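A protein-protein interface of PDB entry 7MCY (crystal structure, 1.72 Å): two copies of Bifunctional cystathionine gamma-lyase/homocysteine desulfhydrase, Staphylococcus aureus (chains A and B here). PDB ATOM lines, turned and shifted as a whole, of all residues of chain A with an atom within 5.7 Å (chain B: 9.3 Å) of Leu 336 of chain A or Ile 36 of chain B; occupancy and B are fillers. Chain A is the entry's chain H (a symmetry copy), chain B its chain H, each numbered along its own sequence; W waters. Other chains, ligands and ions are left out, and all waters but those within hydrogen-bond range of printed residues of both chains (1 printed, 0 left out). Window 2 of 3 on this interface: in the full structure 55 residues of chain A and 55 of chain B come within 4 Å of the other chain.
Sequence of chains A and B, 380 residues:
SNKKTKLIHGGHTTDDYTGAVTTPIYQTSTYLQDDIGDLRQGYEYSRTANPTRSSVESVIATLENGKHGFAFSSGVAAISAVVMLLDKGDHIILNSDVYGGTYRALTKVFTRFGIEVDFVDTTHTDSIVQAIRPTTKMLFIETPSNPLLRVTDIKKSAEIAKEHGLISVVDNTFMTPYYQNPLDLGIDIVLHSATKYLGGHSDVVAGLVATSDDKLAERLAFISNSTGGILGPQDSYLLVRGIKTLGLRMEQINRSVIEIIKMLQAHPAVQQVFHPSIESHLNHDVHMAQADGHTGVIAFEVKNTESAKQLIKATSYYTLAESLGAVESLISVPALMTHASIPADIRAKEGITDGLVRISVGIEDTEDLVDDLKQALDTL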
ATOM      1  N   THR A 305       7.832  12.724  27.242  1.00  0.00           N
ATOM      2  CA  THR A 305       7.590  11.353  26.801  1.00  0.00           C
ATOM      3  C   THR A 305       7.259  10.445  27.977  1.00  0.00           C
ATOM      4  O   THR A 305       6.322   9.641  27.911  1.00  0.00           O
ATOM      5  CB  THR A 305       8.812  10.814  26.053  1.00  0.00           C
ATOM      6  OG1 THR A 305       9.022  11.580  24.865  1.00  0.00           O
ATOM      7  CG2 THR A 305       8.604   9.359  25.667  1.00  0.00           C
ATOM      8  N   LYS A 309       3.878   8.118  28.489  1.00  0.00           N
ATOM      9  CA  LYS A 309       3.884   6.670  28.688  1.00  0.00           C
ATOM     10  C   LYS A 309       3.245   6.291  30.018  1.00  0.00           C
ATOM     11  O   LYS A 309       2.480   5.318  30.093  1.00  0.00           O
ATOM     12  CB  LYS A 309       5.310   6.130  28.604  1.00  0.00           C
ATOM     13  CG  LYS A 309       5.911   6.221  27.210  1.00  0.00           C
ATOM     14  CD  LYS A 309       7.196   5.425  27.107  1.00  0.00           C
ATOM     15  CE  LYS A 309       7.825   5.584  25.732  1.00  0.00           C
ATOM     16  NZ  LYS A 309       9.026   4.720  25.573  1.00  0.00           N
ATOM     17  N   ILE A 312      -0.523   6.542  29.811  1.00  0.00           N
ATOM     18  CA  ILE A 312      -1.077   5.373  29.133  1.00  0.00           C
ATOM     19  C   ILE A 312      -1.122   4.173  30.076  1.00  0.00           C
ATOM     20  O   ILE A 312      -2.114   3.435  30.119  1.00  0.00           O
ATOM     21  CB  ILE A 312      -0.267   5.066  27.860  1.00  0.00           C
ATOM     22  CG1 ILE A 312      -0.489   6.158  26.816  1.00  0.00           C
ATOM     23  CG2 ILE A 312      -0.637   3.707  27.289  1.00  0.00           C
ATOM     24  CD1 ILE A 312       0.442   6.046  25.625  1.00  0.00           C
ATOM     25  N   LEU A 320      -4.199   1.358  24.184  1.00  0.00           N
ATOM     26  CA  LEU A 320      -3.104   1.775  23.314  1.00  0.00           C
ATOM     27  C   LEU A 320      -3.193   0.982  22.017  1.00  0.00           C
ATOM     28  O   LEU A 320      -2.947  -0.231  21.991  1.00  0.00           O
ATOM     29  CB  LEU A 320      -1.751   1.569  23.993  1.00  0.00           C
ATOM     30  CG  LEU A 320      -0.530   1.862  23.117  1.00  0.00           C
ATOM     31  CD1 LEU A 320      -0.478   3.345  22.758  1.00  0.00           C
ATOM     32  CD2 LEU A 320       0.766   1.428  23.809  1.00  0.00           C
ATOM     33  N   VAL A 333       0.457   8.354  21.094  1.00  0.00           N
ATOM     34  CA  VAL A 333       1.427   9.447  21.207  1.00  0.00           C
ATOM     35  C   VAL A 333       1.959   9.733  19.809  1.00  0.00           C
ATOM     36  O   VAL A 333       2.840   9.007  19.329  1.00  0.00           O
ATOM     37  CB  VAL A 333       2.574   9.098  22.172  1.00  0.00           C
ATOM     38  CG1 VAL A 333       3.581  10.268  22.268  1.00  0.00           C
ATOM     39  CG2 VAL A 333       2.026   8.729  23.549  1.00  0.00           C
ATOM     40  N   PRO A 334       1.434  10.750  19.116  1.00  0.00           N
ATOM     41  CA  PRO A 334       1.846  10.990  17.722  1.00  0.00           C
ATOM     42  C   PRO A 334       3.349  11.049  17.514  1.00  0.00           C
ATOM     43  O   PRO A 334       3.839  10.495  16.519  1.00  0.00           O
ATOM     44  CB  PRO A 334       1.178  12.335  17.400  1.00  0.00           C
ATOM     45  CG  PRO A 334      -0.088  12.296  18.226  1.00  0.00           C
ATOM     46  CD  PRO A 334       0.292  11.596  19.512  1.00  0.00           C
ATOM     47  N   ALA A 335       4.097  11.692  18.419  1.00  0.00           N
ATOM     48  CA  ALA A 335       5.537  11.834  18.201  1.00  0.00           C
ATOM     49  C   ALA A 335       6.223  10.483  18.092  1.00  0.00           C
ATOM     50  O   ALA A 335       7.220  10.353  17.378  1.00  0.00           O
ATOM     51  CB  ALA A 335       6.182  12.654  19.320  1.00  0.00           C
ATOM     52  N   LEU A 336       5.696   9.461  18.765  1.00  0.00           N
ATOM     53  CA  LEU A 336       6.298   8.139  18.717  1.00  0.00           C
ATOM     54  C   LEU A 336       5.646   7.207  17.709  1.00  0.00           C
ATOM     55  O   LEU A 336       6.284   6.240  17.281  1.00  0.00           O
ATOM     56  CB  LEU A 336       6.229   7.477  20.100  1.00  0.00           C
ATOM     57  CG  LEU A 336       6.984   8.185  21.224  1.00  0.00           C
ATOM     58  CD1 LEU A 336       6.572   7.612  22.567  1.00  0.00           C
ATOM     59  CD2 LEU A 336       8.483   8.037  21.019  1.00  0.00           C
ATOM     60  N   MET A 337       4.394   7.449  17.340  1.00  0.00           N
ATOM     61  CA  MET A 337       3.635   6.461  16.588  1.00  0.00           C
ATOM     62  C   MET A 337       3.302   6.888  15.172  1.00  0.00           C
ATOM     63  O   MET A 337       3.246   6.038  14.283  1.00  0.00           O
ATOM     64  CB  MET A 337       2.339   6.122  17.333  1.00  0.00           C
ATOM     65  CG  MET A 337       2.608   5.364  18.620  1.00  0.00           C
ATOM     66  SD  MET A 337       1.199   5.207  19.729  1.00  0.00           S
ATOM     67  CE  MET A 337       0.062   4.217  18.751  1.00  0.00           C
ATOM     68  N   THR A 338       3.080   8.169  14.941  1.00  0.00           N
ATOM     69  CA  THR A 338       2.765   8.647  13.611  1.00  0.00           C
ATOM     70  C   THR A 338       3.814   9.587  13.036  1.00  0.00           C
ATOM     71  O   THR A 338       4.056   9.542  11.834  1.00  0.00           O
ATOM     72  CB  THR A 338       1.383   9.329  13.606  1.00  0.00           C
ATOM     73  OG1 THR A 338       1.351  10.390  14.565  1.00  0.00           O
ATOM     74  CG2 THR A 338       0.312   8.325  13.965  1.00  0.00           C
ATOM     75  N   HIS A 339       4.497  10.385  13.856  1.00  0.00           N
ATOM     76  CA  HIS A 339       5.442  11.372  13.344  1.00  0.00           C
ATOM     77  C   HIS A 339       6.883  11.070  13.721  1.00  0.00           C
ATOM     78  O   HIS A 339       7.709  11.989  13.757  1.00  0.00           O
ATOM     79  CB  HIS A 339       5.062  12.768  13.834  1.00  0.00           C
ATOM     80  CG  HIS A 339       3.718  13.219  13.365  1.00  0.00           C
ATOM     81  ND1 HIS A 339       2.548  12.624  13.782  1.00  0.00           N
ATOM     82  CD2 HIS A 339       3.357  14.213  12.520  1.00  0.00           C
ATOM     83  CE1 HIS A 339       1.523  13.228  13.209  1.00  0.00           C
ATOM     84  NE2 HIS A 339       1.987  14.196  12.439  1.00  0.00           N
ATOM     85  N   ALA A 340       7.210   9.807  14.000  1.00  0.00           N
ATOM     86  CA  ALA A 340       8.549   9.494  14.494  1.00  0.00           C
ATOM     87  C   ALA A 340       9.628   9.682  13.436  1.00  0.00           C
ATOM     88  O   ALA A 340      10.805   9.810  13.789  1.00  0.00           O
ATOM     89  CB  ALA A 340       8.599   8.061  15.031  1.00  0.00           C
ATOM     90  N   LEU B  32      -3.916  -4.347  19.771  1.00  0.00           N
ATOM     91  CA  LEU B  32      -3.355  -3.865  21.029  1.00  0.00           C
ATOM     92  C   LEU B  32      -1.839  -3.852  20.967  1.00  0.00           C
ATOM     93  O   LEU B  32      -1.218  -4.793  20.460  1.00  0.00           O
ATOM     94  CB  LEU B  32      -3.786  -4.773  22.185  1.00  0.00           C
ATOM     95  CG  LEU B  32      -5.278  -5.031  22.368  1.00  0.00           C
ATOM     96  CD1 LEU B  32      -5.540  -6.161  23.364  1.00  0.00           C
ATOM     97  CD2 LEU B  32      -5.903  -3.780  22.843  1.00  0.00           C
ATOM     98  N   GLN B  33      -1.240  -2.791  21.507  1.00  0.00           N
ATOM     99  CA  GLN B  33       0.199  -2.733  21.731  1.00  0.00           C
ATOM    100  C   GLN B  33       0.459  -2.741  23.233  1.00  0.00           C
ATOM    101  O   GLN B  33      -0.147  -1.963  23.977  1.00  0.00           O
ATOM    102  CB  GLN B  33       0.806  -1.488  21.079  1.00  0.00           C
ATOM    103  CG  GLN B  33       0.596  -1.457  19.564  1.00  0.00           C
ATOM    104  CD  GLN B  33       1.185  -0.222  18.907  1.00  0.00           C
ATOM    105  OE1 GLN B  33       2.171   0.339  19.384  1.00  0.00           O
ATOM    106  NE2 GLN B  33       0.585   0.203  17.797  1.00  0.00           N
ATOM    107  N   ASP B  34       1.340  -3.639  23.679  1.00  0.00           N
ATOM    108  CA  ASP B  34       1.633  -3.735  25.108  1.00  0.00           C
ATOM    109  C   ASP B  34       2.522  -2.587  25.574  1.00  0.00           C
ATOM    110  O   ASP B  34       2.409  -2.132  26.716  1.00  0.00           O
ATOM    111  CB  ASP B  34       2.273  -5.091  25.408  1.00  0.00           C
ATOM    112  CG  ASP B  34       1.308  -6.243  25.174  1.00  0.00           C
ATOM    113  OD1 ASP B  34       0.127  -6.095  25.552  1.00  0.00           O
ATOM    114  OD2 ASP B  34       1.714  -7.275  24.601  1.00  0.00           O
ATOM    115  N   ASP B  35       3.398  -2.111  24.703  1.00  0.00           N
ATOM    116  CA  ASP B  35       4.149  -0.881  24.896  1.00  0.00           C
ATOM    117  C   ASP B  35       4.204  -0.203  23.543  1.00  0.00           C
ATOM    118  O   ASP B  35       4.061  -0.861  22.511  1.00  0.00           O
ATOM    119  CB  ASP B  35       5.572  -1.137  25.415  1.00  0.00           C
ATOM    120  CG  ASP B  35       5.585  -1.715  26.812  1.00  0.00           C
ATOM    121  OD1 ASP B  35       5.456  -0.934  27.780  1.00  0.00           O
ATOM    122  OD2 ASP B  35       5.718  -2.952  26.943  1.00  0.00           O
ATOM    123  N   ILE B  36       4.421   1.113  23.544  1.00  0.00           N
ATOM    124  CA  ILE B  36       4.420   1.837  22.277  1.00  0.00           C
ATOM    125  C   ILE B  36       5.475   1.235  21.365  1.00  0.00           C
ATOM    126  O   ILE B  36       6.663   1.191  21.711  1.00  0.00           O
ATOM    127  CB  ILE B  36       4.655   3.333  22.495  1.00  0.00           C
ATOM    128  CG1 ILE B  36       3.461   3.963  23.204  1.00  0.00           C
ATOM    129  CG2 ILE B  36       4.898   4.016  21.155  1.00  0.00           C
ATOM    130  CD1 ILE B  36       3.673   5.417  23.565  1.00  0.00           C
ATOM    131  N   GLY B  37       5.041   0.733  20.205  1.00  0.00           N
ATOM    132  CA  GLY B  37       5.939   0.170  19.222  1.00  0.00           C
ATOM    133  C   GLY B  37       6.198  -1.316  19.351  1.00  0.00           C
ATOM    134  O   GLY B  37       6.813  -1.901  18.448  1.00  0.00           O
ATOM    135  N   ASP B  38       5.774  -1.948  20.440  1.00  0.00           N
ATOM    136  CA  ASP B  38       5.944  -3.385  20.615  1.00  0.00           C
ATOM    137  C   ASP B  38       4.677  -4.083  20.132  1.00  0.00           C
ATOM    138  O   ASP B  38       3.627  -4.005  20.783  1.00  0.00           O
ATOM    139  CB  ASP B  38       6.243  -3.719  22.074  1.00  0.00           C
ATOM    140  CG  ASP B  38       7.615  -3.232  22.516  1.00  0.00           C
ATOM    141  OD1 ASP B  38       8.319  -2.612  21.693  1.00  0.00           O
ATOM    142  OD2 ASP B  38       7.986  -3.471  23.685  1.00  0.00           O
ATOM    143  N   LEU B  39       4.777  -4.764  18.996  1.00  0.00           N
ATOM    144  CA  LEU B  39       3.669  -5.516  18.427  1.00  0.00           C
ATOM    145  C   LEU B  39       3.782  -6.966  18.874  1.00  0.00           C
ATOM    146  O   LEU B  39       4.844  -7.578  18.726  1.00  0.00           O
ATOM    147  CB  LEU B  39       3.702  -5.413  16.899  1.00  0.00           C
ATOM    148  CG  LEU B  39       3.928  -4.003  16.340  1.00  0.00           C
ATOM    149  CD1 LEU B  39       3.945  -3.990  14.809  1.00  0.00           C
ATOM    150  CD2 LEU B  39       2.867  -3.038  16.875  1.00  0.00           C
ATOM    151  N   GLU B  44      -0.200  -4.373  13.502  1.00  0.00           N
ATOM    152  CA  GLU B  44      -0.536  -3.080  14.084  1.00  0.00           C
ATOM    153  C   GLU B  44      -1.720  -2.392  13.419  1.00  0.00           C
ATOM    154  O   GLU B  44      -2.417  -1.634  14.100  1.00  0.00           O
ATOM    155  CB  GLU B  44       0.688  -2.146  14.058  1.00  0.00           C
ATOM    156  CG  GLU B  44       0.867  -1.350  12.806  1.00  0.00           C
ATOM    157  CD  GLU B  44       2.195  -0.593  12.779  1.00  0.00           C
ATOM    158  OE1 GLU B  44       3.016  -0.889  11.895  1.00  0.00           O
ATOM    159  OE2 GLU B  44       2.417   0.288  13.637  1.00  0.00           O
HETATM  160  O   HOH W   1       7.970   1.733  24.252  1.00  0.00           O
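The backbone carbonyl oxygen (O) of Leu 320 of chain A lies within hydrogen-bond range of the backbone NH (N) of Gln 33 of chain B (3.1 Å).
The backbone NH of Val 333 of chain A sits at hydrogen-bond distance from the side-chain sulfur of Met 337 of chain A (3.5 Å). The side-chain amide oxygen (OE1) of Gln 33 of chain B sits at hydrogen-bond distance from the backbone NH (N) of Gly 37 of chain B.
Among the printed residues, pairs that only touch across the chains: Met 337 of chain A with Ile 36 of chain B (3.7 Å), Leu 320 of chain A with Ile 36 of chain B (3.7 Å), Val 333 of chain A with Ile 36 of chain B (3.7 Å), Leu 336 of chain A with Ile 36 of chain B (3.8 Å), Leu 320 of chain A with Leu 32 of chain B (3.8 Å), Leu 320 of chain A with Asp 35 of chain B (3.8 Å) and Ile 312 of chain A with Ile 36 of chain B (3.9 Å).
Of the printed residues of chain B, Leu 336 of chain A touches Ile 36. Val 333 of chain A touches just one residue of chain B: Ile 36. Of the printed residues of chain A, Leu 32 of chain B touches Leu 320. Of the printed residues of chain B, Leu 320 of chain A touches Leu 32 (3.8 Å), Gln 33 (3.1 Å), Asp 35 (3.8 Å) and Ile 36 (3.7 Å). Of the printed residues of chain A, Asp 35 of chain B touches Leu 320 (3.8 Å). Lys 309 of chain A touches none of the printed residues of chain B. Gly 37 of chain B touches none of the printed residues of chain A. The nearest residue of chain B that does not touch Leu 336 of chain A is Gly 37 of chain B (6.4 Å). The nearest printed residue of chain B that does not touch Ile 312 of chain A is Gln 33 of chain B (6.6 Å).
Of the 12 printed residues of chain A, 5 touch a printed residue of chain B. Printed residues of chain A that touch a printed residue of chain B: Ile 312, Leu 320, Val 333, Leu 336 and Met 337. Hydrophobic or aromatic side chains of chain A within 4 Å of the printed part of chain B: Ile 312, Leu 320, Val 333, Leu 336 and Met 337. Printed residues of chain B that touch a printed residue of chain A: Leu 32, Gln 33, Asp 35 and Ile 36. Hydrophobic or aromatic side chains of chain B that line the printed part of chain A: Ile 36. Among the printed residues, no Asp or Glu carboxylate lies within 4 Å of a Lys or Arg side-chain nitrogen of the other chain.
No position is printed for both chains.
Water W1 bridges the backbone carbonyl oxygen of Ile 36 of chain B (2.9 Å) and the side-chain amino group of Lys 309 of chain A (3.4 Å).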
